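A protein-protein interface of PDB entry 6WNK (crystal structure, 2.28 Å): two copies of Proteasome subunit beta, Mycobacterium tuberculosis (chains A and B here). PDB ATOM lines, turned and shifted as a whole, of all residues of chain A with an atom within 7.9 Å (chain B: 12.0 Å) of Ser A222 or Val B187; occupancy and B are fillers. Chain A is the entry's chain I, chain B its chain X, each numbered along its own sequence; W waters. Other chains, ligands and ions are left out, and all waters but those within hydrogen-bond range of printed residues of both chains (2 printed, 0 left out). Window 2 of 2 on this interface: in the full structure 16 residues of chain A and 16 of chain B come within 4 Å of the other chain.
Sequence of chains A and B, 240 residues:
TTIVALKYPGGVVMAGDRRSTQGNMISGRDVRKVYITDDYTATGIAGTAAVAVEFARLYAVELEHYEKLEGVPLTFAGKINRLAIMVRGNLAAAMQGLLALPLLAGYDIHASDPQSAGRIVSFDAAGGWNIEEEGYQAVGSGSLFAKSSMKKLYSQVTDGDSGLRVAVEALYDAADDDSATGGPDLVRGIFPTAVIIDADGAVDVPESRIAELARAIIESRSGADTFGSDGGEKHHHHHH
The side-chain carboxylate of Asp A176 is in salt-bridge range of the guanidinium group of Arg B29, at 3.7 Å.
The side-chain carboxylate (OD2) of Asp A176 lies within salt-bridge range of the guanidinium group (NH1) of Arg B188 (2.8 Å).
The backbone carbonyl oxygen of Ile A218 is in hydrogen-bond range of the side-chain hydroxyl of Ser A222 (2.9 Å).
The side-chain carboxylate of Asp B185 sits at hydrogen-bond distance from the backbone NH of Val B187, 3.2 Å away.
The side-chain carboxylate of Asp B185 lies within salt-bridge range of the guanidinium group of Arg B188.
OH of Tyr A172 touches CG2 of Val B187, 3.6 Å away.
Ile A218 touches Val B187.
Arg A221 touches Val B187 (CB to CG1, 3.6 Å).
CA of Ser A222 touches O of Val B187, at 3.7 Å.
Ser A222 touches just one residue of chain B: Val B187 (3.7 Å).
Val B187 touches just these residues of chain A: Tyr A172 (3.6 Å), Ile A218 (3.7 Å), Arg A221 (3.6 Å) and Ser A222 (3.7 Å).
No residue of chain B comes within 4 Å of Glu A219.
No residue of chain B comes within 4 Å of Ser A220.
Printed residues of chain A within 4 Å of Arg B188: Asp A176 (2.8 Å).
Printed residues of chain B within 4 Å of Arg A221: Val B187.
Of the printed residues of chain A, Arg B29 touches Asp A176 (2.6 Å).
Printed residues of chain B within 4 Å of Asp A176: Arg B29 and Arg B188.
Arg A215 touches none of the printed residues of chain B.
The nearest residue of chain B that does not touch Ser A222 is Leu B186 (4.8 Å).
The nearest residue of chain A that does not touch Val B187 is Glu A219 (6.2 Å).
Of the 20 printed residues of chain B, 3 touch a printed residue of chain A.
Hydrophobic or aromatic side chains of chain B that line the printed part of chain A: Val B187.
Printed residues of chain A that touch a printed residue of chain B: Tyr A172, Asp A176, Ile A218, Arg A221 and Ser A222.
Among the printed residues, Asp or Glu carboxylates within 4 Å of a Lys or Arg side-chain nitrogen of the other chain: Asp A176 with Arg B29 (3.7 Å) and Asp A176 with Arg B188 (2.8 Å).
Positions printed for both chains: 172, 186, 215 and 218.
Of the 6 pairs that touch across the chains among the printed residues, none has its exchanged pair printed and touching as well.
Water W2 lies within hydrogen-bond range of NE of Arg B29 and OD1 of Asp A176.
Water W1 lies within hydrogen-bond range of OD1 of Asp A176 and NH2 of Arg B188.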
ATOM      1  N   TYR A 172     -21.577 -13.779  25.477  1.00  0.00           N
ATOM      2  CA  TYR A 172     -21.780 -12.695  24.527  1.00  0.00           C
ATOM      3  C   TYR A 172     -22.994 -12.968  23.647  1.00  0.00           C
ATOM      4  O   TYR A 172     -23.827 -12.083  23.423  1.00  0.00           O
ATOM      5  CB  TYR A 172     -20.523 -12.499  23.678  1.00  0.00           C
ATOM      6  CG  TYR A 172     -20.592 -11.259  22.823  1.00  0.00           C
ATOM      7  CD1 TYR A 172     -20.183 -10.030  23.323  1.00  0.00           C
ATOM      8  CD2 TYR A 172     -21.091 -11.308  21.525  1.00  0.00           C
ATOM      9  CE1 TYR A 172     -20.255  -8.885  22.557  1.00  0.00           C
ATOM     10  CE2 TYR A 172     -21.169 -10.162  20.745  1.00  0.00           C
ATOM     11  CZ  TYR A 172     -20.746  -8.957  21.272  1.00  0.00           C
ATOM     12  OH  TYR A 172     -20.819  -7.813  20.516  1.00  0.00           O
ATOM     13  N   ASP A 176     -26.544 -11.031  23.362  1.00  0.00           N
ATOM     14  CA  ASP A 176     -26.939 -10.548  22.046  1.00  0.00           C
ATOM     15  C   ASP A 176     -28.432 -10.740  21.803  1.00  0.00           C
ATOM     16  O   ASP A 176     -29.059  -9.932  21.108  1.00  0.00           O
ATOM     17  CB  ASP A 176     -26.123 -11.284  20.980  1.00  0.00           C
ATOM     18  CG  ASP A 176     -25.880 -10.448  19.748  1.00  0.00           C
ATOM     19  OD1 ASP A 176     -26.101  -9.219  19.803  1.00  0.00           O
ATOM     20  OD2 ASP A 176     -25.464 -11.023  18.722  1.00  0.00           O
ATOM     21  N   LEU A 186     -18.007  -1.945  27.755  1.00  0.00           N
ATOM     22  CA  LEU A 186     -16.708  -1.331  27.501  1.00  0.00           C
ATOM     23  C   LEU A 186     -16.639   0.102  28.010  1.00  0.00           C
ATOM     24  O   LEU A 186     -15.537   0.608  28.247  1.00  0.00           O
ATOM     25  CB  LEU A 186     -16.382  -1.357  26.007  1.00  0.00           C
ATOM     26  CG  LEU A 186     -16.465  -2.701  25.283  1.00  0.00           C
ATOM     27  CD1 LEU A 186     -15.868  -2.584  23.886  1.00  0.00           C
ATOM     28  CD2 LEU A 186     -15.772  -3.791  26.075  1.00  0.00           C
ATOM     29  N   ARG A 215     -13.052  -8.161  24.245  1.00  0.00           N
ATOM     30  CA  ARG A 215     -12.771  -7.183  23.197  1.00  0.00           C
ATOM     31  C   ARG A 215     -12.379  -7.875  21.898  1.00  0.00           C
ATOM     32  O   ARG A 215     -12.760  -7.427  20.811  1.00  0.00           O
ATOM     33  CB  ARG A 215     -11.695  -6.199  23.652  1.00  0.00           C
ATOM     34  CG  ARG A 215     -12.266  -5.037  24.459  1.00  0.00           C
ATOM     35  CD  ARG A 215     -11.212  -3.998  24.806  1.00  0.00           C
ATOM     36  NE  ARG A 215     -10.817  -4.090  26.207  1.00  0.00           N
ATOM     37  CZ  ARG A 215     -11.332  -3.344  27.178  1.00  0.00           C
ATOM     38  NH1 ARG A 215     -12.255  -2.432  26.898  1.00  0.00           N
ATOM     39  NH2 ARG A 215     -10.916  -3.505  28.427  1.00  0.00           N
ATOM     40  N   ALA A 216     -11.636  -8.980  21.992  1.00  0.00           N
ATOM     41  CA  ALA A 216     -11.308  -9.748  20.794  1.00  0.00           C
ATOM     42  C   ALA A 216     -12.567 -10.317  20.143  1.00  0.00           C
ATOM     43  O   ALA A 216     -12.700 -10.297  18.912  1.00  0.00           O
ATOM     44  CB  ALA A 216     -10.318 -10.862  21.141  1.00  0.00           C
ATOM     45  N   ILE A 217     -13.512 -10.801  20.951  1.00  0.00           N
ATOM     46  CA  ILE A 217     -14.781 -11.278  20.404  1.00  0.00           C
ATOM     47  C   ILE A 217     -15.519 -10.138  19.714  1.00  0.00           C
ATOM     48  O   ILE A 217     -16.034 -10.290  18.601  1.00  0.00           O
ATOM     49  CB  ILE A 217     -15.635 -11.920  21.511  1.00  0.00           C
ATOM     50  CG1 ILE A 217     -15.033 -13.266  21.927  1.00  0.00           C
ATOM     51  CG2 ILE A 217     -17.084 -12.081  21.047  1.00  0.00           C
ATOM     52  CD1 ILE A 217     -15.409 -13.704  23.325  1.00  0.00           C
ATOM     53  N   ILE A 218     -15.568  -8.972  20.362  1.00  0.00           N
ATOM     54  CA  ILE A 218     -16.280  -7.833  19.793  1.00  0.00           C
ATOM     55  C   ILE A 218     -15.619  -7.384  18.493  1.00  0.00           C
ATOM     56  O   ILE A 218     -16.300  -7.042  17.516  1.00  0.00           O
ATOM     57  CB  ILE A 218     -16.358  -6.691  20.825  1.00  0.00           C
ATOM     58  CG1 ILE A 218     -17.255  -7.102  21.995  1.00  0.00           C
ATOM     59  CG2 ILE A 218     -16.873  -5.410  20.180  1.00  0.00           C
ATOM     60  CD1 ILE A 218     -17.237  -6.136  23.157  1.00  0.00           C
ATOM     61  N   GLU A 219     -14.285  -7.401  18.453  1.00  0.00           N
ATOM     62  CA  GLU A 219     -13.573  -7.023  17.235  1.00  0.00           C
ATOM     63  C   GLU A 219     -13.837  -8.015  16.107  1.00  0.00           C
ATOM     64  O   GLU A 219     -14.062  -7.616  14.959  1.00  0.00           O
ATOM     65  CB  GLU A 219     -12.074  -6.914  17.522  1.00  0.00           C
ATOM     66  CG  GLU A 219     -11.293  -6.179  16.449  1.00  0.00           C
ATOM     67  CD  GLU A 219     -11.661  -4.706  16.364  1.00  0.00           C
ATOM     68  OE1 GLU A 219     -11.509  -3.993  17.381  1.00  0.00           O
ATOM     69  OE2 GLU A 219     -12.110  -4.267  15.281  1.00  0.00           O
ATOM     70  N   SER A 220     -13.823  -9.313  16.417  1.00  0.00           N
ATOM     71  CA  SER A 220     -14.112 -10.323  15.406  1.00  0.00           C
ATOM     72  C   SER A 220     -15.524 -10.177  14.840  1.00  0.00           C
ATOM     73  O   SER A 220     -15.745 -10.432  13.650  1.00  0.00           O
ATOM     74  CB  SER A 220     -13.917 -11.716  16.001  1.00  0.00           C
ATOM     75  OG  SER A 220     -14.619 -12.693  15.257  1.00  0.00           O
ATOM     76  N   ARG A 221     -16.491  -9.766  15.667  1.00  0.00           N
ATOM     77  CA  ARG A 221     -17.869  -9.648  15.202  1.00  0.00           C
ATOM     78  C   ARG A 221     -18.090  -8.433  14.308  1.00  0.00           C
ATOM     79  O   ARG A 221     -19.018  -8.443  13.492  1.00  0.00           O
ATOM     80  CB  ARG A 221     -18.831  -9.585  16.393  1.00  0.00           C
ATOM     81  CG  ARG A 221     -18.873 -10.842  17.262  1.00  0.00           C
ATOM     82  CD  ARG A 221     -19.606 -11.986  16.580  1.00  0.00           C
ATOM     83  NE  ARG A 221     -19.496 -13.232  17.339  1.00  0.00           N
ATOM     84  CZ  ARG A 221     -20.414 -13.678  18.191  1.00  0.00           C
ATOM     85  NH1 ARG A 221     -21.525 -12.985  18.399  1.00  0.00           N
ATOM     86  NH2 ARG A 221     -20.224 -14.825  18.833  1.00  0.00           N
ATOM     87  N   SER A 222     -17.261  -7.402  14.431  1.00  0.00           N
ATOM     88  CA  SER A 222     -17.455  -6.161  13.686  1.00  0.00           C
ATOM     89  C   SER A 222     -17.089  -6.304  12.211  1.00  0.00           C
ATOM     90  O   SER A 222     -16.047  -6.863  11.875  1.00  0.00           O
ATOM     91  CB  SER A 222     -16.634  -5.038  14.317  1.00  0.00           C
ATOM     92  OG  SER A 222     -16.945  -4.906  15.692  1.00  0.00           O
ATOM     93  N   ARG B  19     -34.985  -0.911  18.643  1.00  0.00           N
ATOM     94  CA  ARG B  19     -35.157  -2.237  19.221  1.00  0.00           C
ATOM     95  C   ARG B  19     -36.620  -2.663  19.210  1.00  0.00           C
ATOM     96  O   ARG B  19     -37.519  -1.853  19.453  1.00  0.00           O
ATOM     97  CB  ARG B  19     -34.617  -2.272  20.652  1.00  0.00           C
ATOM     98  CG  ARG B  19     -34.933  -3.556  21.420  1.00  0.00           C
ATOM     99  CD  ARG B  19     -34.056  -3.701  22.655  1.00  0.00           C
ATOM    100  NE  ARG B  19     -32.647  -3.809  22.284  1.00  0.00           N
ATOM    101  CZ  ARG B  19     -31.657  -3.994  23.151  1.00  0.00           C
ATOM    102  NH1 ARG B  19     -31.917  -4.090  24.450  1.00  0.00           N
ATOM    103  NH2 ARG B  19     -30.407  -4.084  22.717  1.00  0.00           N
ATOM    104  N   ARG B  29     -33.480  -5.367  15.640  1.00  0.00           N
ATOM    105  CA  ARG B  29     -32.373  -4.450  15.856  1.00  0.00           C
ATOM    106  C   ARG B  29     -32.385  -3.261  14.911  1.00  0.00           C
ATOM    107  O   ARG B  29     -31.612  -2.321  15.121  1.00  0.00           O
ATOM    108  CB  ARG B  29     -31.032  -5.185  15.703  1.00  0.00           C
ATOM    109  CG  ARG B  29     -30.961  -6.480  16.482  1.00  0.00           C
ATOM    110  CD  ARG B  29     -29.556  -7.048  16.508  1.00  0.00           C
ATOM    111  NE  ARG B  29     -29.398  -7.990  17.612  1.00  0.00           N
ATOM    112  CZ  ARG B  29     -29.588  -9.301  17.509  1.00  0.00           C
ATOM    113  NH1 ARG B  29     -29.933  -9.835  16.348  1.00  0.00           N
ATOM    114  NH2 ARG B  29     -29.430 -10.077  18.566  1.00  0.00           N
ATOM    115  N   ASP B  30     -33.252  -3.270  13.899  1.00  0.00           N
ATOM    116  CA  ASP B  30     -33.238  -2.304  12.808  1.00  0.00           C
ATOM    117  C   ASP B  30     -34.536  -1.515  12.700  1.00  0.00           C
ATOM    118  O   ASP B  30     -34.755  -0.858  11.672  1.00  0.00           O
ATOM    119  CB  ASP B  30     -32.985  -3.020  11.476  1.00  0.00           C
ATOM    120  CG  ASP B  30     -31.623  -3.671  11.408  1.00  0.00           C
ATOM    121  OD1 ASP B  30     -30.623  -2.931  11.309  1.00  0.00           O
ATOM    122  OD2 ASP B  30     -31.546  -4.919  11.453  1.00  0.00           O
ATOM    123  N   TYR B 172     -29.570   7.672  24.521  1.00  0.00           N
ATOM    124  CA  TYR B 172     -28.501   6.874  25.116  1.00  0.00           C
ATOM    125  C   TYR B 172     -28.766   6.612  26.597  1.00  0.00           C
ATOM    126  O   TYR B 172     -28.565   5.493  27.082  1.00  0.00           O
ATOM    127  CB  TYR B 172     -27.152   7.573  24.933  1.00  0.00           C
ATOM    128  CG  TYR B 172     -25.974   6.720  25.365  1.00  0.00           C
ATOM    129  CD1 TYR B 172     -25.537   6.706  26.687  1.00  0.00           C
ATOM    130  CD2 TYR B 172     -25.308   5.920  24.449  1.00  0.00           C
ATOM    131  CE1 TYR B 172     -24.461   5.916  27.075  1.00  0.00           C
ATOM    132  CE2 TYR B 172     -24.242   5.132  24.824  1.00  0.00           C
ATOM    133  CZ  TYR B 172     -23.822   5.131  26.133  1.00  0.00           C
ATOM    134  OH  TYR B 172     -22.756   4.338  26.487  1.00  0.00           O
ATOM    135  N   GLY B 182     -33.102   0.240  22.697  1.00  0.00           N
ATOM    136  CA  GLY B 182     -31.817  -0.188  22.163  1.00  0.00           C
ATOM    137  C   GLY B 182     -30.790   0.934  22.165  1.00  0.00           C
ATOM    138  O   GLY B 182     -31.076   2.056  21.737  1.00  0.00           O
ATOM    139  N   GLY B 183     -29.590   0.628  22.652  1.00  0.00           N
ATOM    140  CA  GLY B 183     -28.482   1.549  22.558  1.00  0.00           C
ATOM    141  C   GLY B 183     -27.854   1.527  21.183  1.00  0.00           C
ATOM    142  O   GLY B 183     -28.230   0.743  20.299  1.00  0.00           O
ATOM    143  N   PRO B 184     -26.884   2.417  20.972  1.00  0.00           N
ATOM    144  CA  PRO B 184     -26.103   2.356  19.731  1.00  0.00           C
ATOM    145  C   PRO B 184     -25.356   1.032  19.635  1.00  0.00           C
ATOM    146  O   PRO B 184     -24.787   0.544  20.614  1.00  0.00           O
ATOM    147  CB  PRO B 184     -25.142   3.545  19.854  1.00  0.00           C
ATOM    148  CG  PRO B 184     -25.792   4.467  20.834  1.00  0.00           C
ATOM    149  CD  PRO B 184     -26.523   3.580  21.802  1.00  0.00           C
ATOM    150  N   ASP B 185     -25.382   0.440  18.445  1.00  0.00           N
ATOM    151  CA  ASP B 185     -24.758  -0.856  18.183  1.00  0.00           C
ATOM    152  C   ASP B 185     -23.527  -0.608  17.317  1.00  0.00           C
ATOM    153  O   ASP B 185     -23.637  -0.437  16.101  1.00  0.00           O
ATOM    154  CB  ASP B 185     -25.746  -1.804  17.504  1.00  0.00           C
ATOM    155  CG  ASP B 185     -25.240  -3.234  17.429  1.00  0.00           C
ATOM    156  OD1 ASP B 185     -24.012  -3.456  17.533  1.00  0.00           O
ATOM    157  OD2 ASP B 185     -26.082  -4.141  17.264  1.00  0.00           O
ATOM    158  N   LEU B 186     -22.353  -0.591  17.947  1.00  0.00           N
ATOM    159  CA  LEU B 186     -21.130  -0.309  17.204  1.00  0.00           C
ATOM    160  C   LEU B 186     -20.662  -1.510  16.391  1.00  0.00           C
ATOM    161  O   LEU B 186     -20.062  -1.328  15.326  1.00  0.00           O
ATOM    162  CB  LEU B 186     -20.025   0.140  18.160  1.00  0.00           C
ATOM    163  CG  LEU B 186     -20.340   1.380  18.997  1.00  0.00           C
ATOM    164  CD1 LEU B 186     -19.130   1.783  19.827  1.00  0.00           C
ATOM    165  CD2 LEU B 186     -20.801   2.527  18.111  1.00  0.00           C
ATOM    166  N   VAL B 187     -20.921  -2.729  16.870  1.00  0.00           N
ATOM    167  CA  VAL B 187     -20.531  -3.924  16.124  1.00  0.00           C
ATOM    168  C   VAL B 187     -21.248  -3.969  14.780  1.00  0.00           C
ATOM    169  O   VAL B 187     -20.626  -4.173  13.733  1.00  0.00           O
ATOM    170  CB  VAL B 187     -20.810  -5.192  16.951  1.00  0.00           C
ATOM    171  CG1 VAL B 187     -20.484  -6.436  16.137  1.00  0.00           C
ATOM    172  CG2 VAL B 187     -20.018  -5.173  18.252  1.00  0.00           C
ATOM    173  N   ARG B 188     -22.568  -3.769  14.794  1.00  0.00           N
ATOM    174  CA  ARG B 188     -23.389  -3.817  13.590  1.00  0.00           C
ATOM    175  C   ARG B 188     -23.509  -2.472  12.889  1.00  0.00           C
ATOM    176  O   ARG B 188     -24.000  -2.424  11.756  1.00  0.00           O
ATOM    177  CB  ARG B 188     -24.795  -4.329  13.930  1.00  0.00           C
ATOM    178  CG  ARG B 188     -24.828  -5.732  14.542  1.00  0.00           C
ATOM    179  CD  ARG B 188     -26.258  -6.171  14.864  1.00  0.00           C
ATOM    180  NE  ARG B 188     -26.330  -7.597  15.164  1.00  0.00           N
ATOM    181  CZ  ARG B 188     -26.175  -8.119  16.376  1.00  0.00           C
ATOM    182  NH1 ARG B 188     -26.247  -9.432  16.542  1.00  0.00           N
ATOM    183  NH2 ARG B 188     -25.948  -7.333  17.421  1.00  0.00           N
ATOM    184  N   GLY B 189     -23.088  -1.384  13.526  1.00  0.00           N
ATOM    185  CA  GLY B 189     -23.253  -0.071  12.937  1.00  0.00           C
ATOM    186  C   GLY B 189     -24.707   0.329  12.794  1.00  0.00           C
ATOM    187  O   GLY B 189     -25.109   0.839  11.747  1.00  0.00           O
ATOM    188  N   ILE B 190     -25.508   0.101  13.834  1.00  0.00           N
ATOM    189  CA  ILE B 190     -26.920   0.476  13.853  1.00  0.00           C
ATOM    190  C   ILE B 190     -27.119   1.543  14.916  1.00  0.00           C
ATOM    191  O   ILE B 190     -26.703   1.368  16.068  1.00  0.00           O
ATOM    192  CB  ILE B 190     -27.831  -0.732  14.126  1.00  0.00           C
ATOM    193  CG1 ILE B 190     -27.602  -1.819  13.080  1.00  0.00           C
ATOM    194  CG2 ILE B 190     -29.301  -0.302  14.135  1.00  0.00           C
ATOM    195  CD1 ILE B 190     -28.340  -3.101  13.390  1.00  0.00           C
ATOM    196  N   PHE B 191     -27.770   2.635  14.541  1.00  0.00           N
ATOM    197  CA  PHE B 191     -27.916   3.798  15.399  1.00  0.00           C
ATOM    198  C   PHE B 191     -29.353   4.287  15.379  1.00  0.00           C
ATOM    199  O   PHE B 191     -30.111   3.978  14.454  1.00  0.00           O
ATOM    200  CB  PHE B 191     -26.965   4.916  14.948  1.00  0.00           C
ATOM    201  CG  PHE B 191     -25.523   4.513  14.991  1.00  0.00           C
ATOM    202  CD1 PHE B 191     -24.798   4.622  16.168  1.00  0.00           C
ATOM    203  CD2 PHE B 191     -24.907   3.974  13.873  1.00  0.00           C
ATOM    204  CE1 PHE B 191     -23.477   4.228  16.222  1.00  0.00           C
ATOM    205  CE2 PHE B 191     -23.582   3.575  13.920  1.00  0.00           C
ATOM    206  CZ  PHE B 191     -22.866   3.703  15.095  1.00  0.00           C
ATOM    207  N   PRO B 192     -29.769   5.033  16.405  1.00  0.00           N
ATOM    208  CA  PRO B 192     -31.109   5.629  16.391  1.00  0.00           C
ATOM    209  C   PRO B 192     -31.337   6.446  15.125  1.00  0.00           C
ATOM    210  O   PRO B 192     -30.397   6.959  14.515  1.00  0.00           O
ATOM    211  CB  PRO B 192     -31.114   6.519  17.638  1.00  0.00           C
ATOM    212  CG  PRO B 192     -30.122   5.875  18.559  1.00  0.00           C
ATOM    213  CD  PRO B 192     -29.055   5.294  17.671  1.00  0.00           C
ATOM    214  N   GLU B 207     -27.540   8.762   8.790  1.00  0.00           N
ATOM    215  CA  GLU B 207     -27.040   7.855   9.816  1.00  0.00           C
ATOM    216  C   GLU B 207     -25.645   8.247  10.287  1.00  0.00           C
ATOM    217  O   GLU B 207     -25.332   8.106  11.475  1.00  0.00           O
ATOM    218  CB  GLU B 207     -27.039   6.421   9.280  1.00  0.00           C
ATOM    219  CG  GLU B 207     -26.449   5.383  10.226  1.00  0.00           C
ATOM    220  CD  GLU B 207     -26.071   4.092   9.513  1.00  0.00           C
ATOM    221  OE1 GLU B 207     -25.764   4.146   8.301  1.00  0.00           O
ATOM    222  OE2 GLU B 207     -26.080   3.021  10.161  1.00  0.00           O
ATOM    223  N   ALA B 211     -24.261   8.404  14.069  1.00  0.00           N
ATOM    224  CA  ALA B 211     -23.104   7.595  14.442  1.00  0.00           C
ATOM    225  C   ALA B 211     -22.030   8.448  15.105  1.00  0.00           C
ATOM    226  O   ALA B 211     -21.474   8.071  16.146  1.00  0.00           O
ATOM    227  CB  ALA B 211     -22.540   6.886  13.210  1.00  0.00           C
ATOM    228  N   ALA B 214     -23.245   9.419  18.593  1.00  0.00           N
ATOM    229  CA  ALA B 214     -23.262   8.253  19.470  1.00  0.00           C
ATOM    230  C   ALA B 214     -21.855   7.891  19.934  1.00  0.00           C
ATOM    231  O   ALA B 214     -21.620   7.672  21.131  1.00  0.00           O
ATOM    232  CB  ALA B 214     -23.921   7.070  18.757  1.00  0.00           C
ATOM    233  N   ARG B 215     -20.901   7.837  18.998  1.00  0.00           N
ATOM    234  CA  ARG B 215     -19.522   7.525  19.370  1.00  0.00           C
ATOM    235  C   ARG B 215     -18.940   8.575  20.307  1.00  0.00           C
ATOM    236  O   ARG B 215     -18.149   8.240  21.194  1.00  0.00           O
ATOM    237  CB  ARG B 215     -18.649   7.398  18.117  1.00  0.00           C
ATOM    238  CG  ARG B 215     -19.049   6.262  17.184  1.00  0.00           C
ATOM    239  CD  ARG B 215     -18.100   6.156  15.999  1.00  0.00           C
ATOM    240  NE  ARG B 215     -18.766   5.632  14.809  1.00  0.00           N
ATOM    241  CZ  ARG B 215     -18.809   4.345  14.477  1.00  0.00           C
ATOM    242  NH1 ARG B 215     -18.218   3.436  15.247  1.00  0.00           N
ATOM    243  NH2 ARG B 215     -19.445   3.969  13.372  1.00  0.00           N
ATOM    244  N   ILE B 218     -20.271   7.873  23.818  1.00  0.00           N
ATOM    245  CA  ILE B 218     -19.589   6.692  24.342  1.00  0.00           C
ATOM    246  C   ILE B 218     -18.159   7.036  24.742  1.00  0.00           C
ATOM    247  O   ILE B 218     -17.695   6.675  25.830  1.00  0.00           O
ATOM    248  CB  ILE B 218     -19.629   5.552  23.308  1.00  0.00           C
ATOM    249  CG1 ILE B 218     -21.050   4.989  23.195  1.00  0.00           C
ATOM    250  CG2 ILE B 218     -18.631   4.468  23.669  1.00  0.00           C
ATOM    251  CD1 ILE B 218     -21.283   4.145  21.963  1.00  0.00           C
HETATM  252  O   HOH W   1     -26.000  -6.466  20.776  1.00  0.00           O
HETATM  253  O   HOH W   2     -28.224  -7.227  20.158  1.00  0.00           O
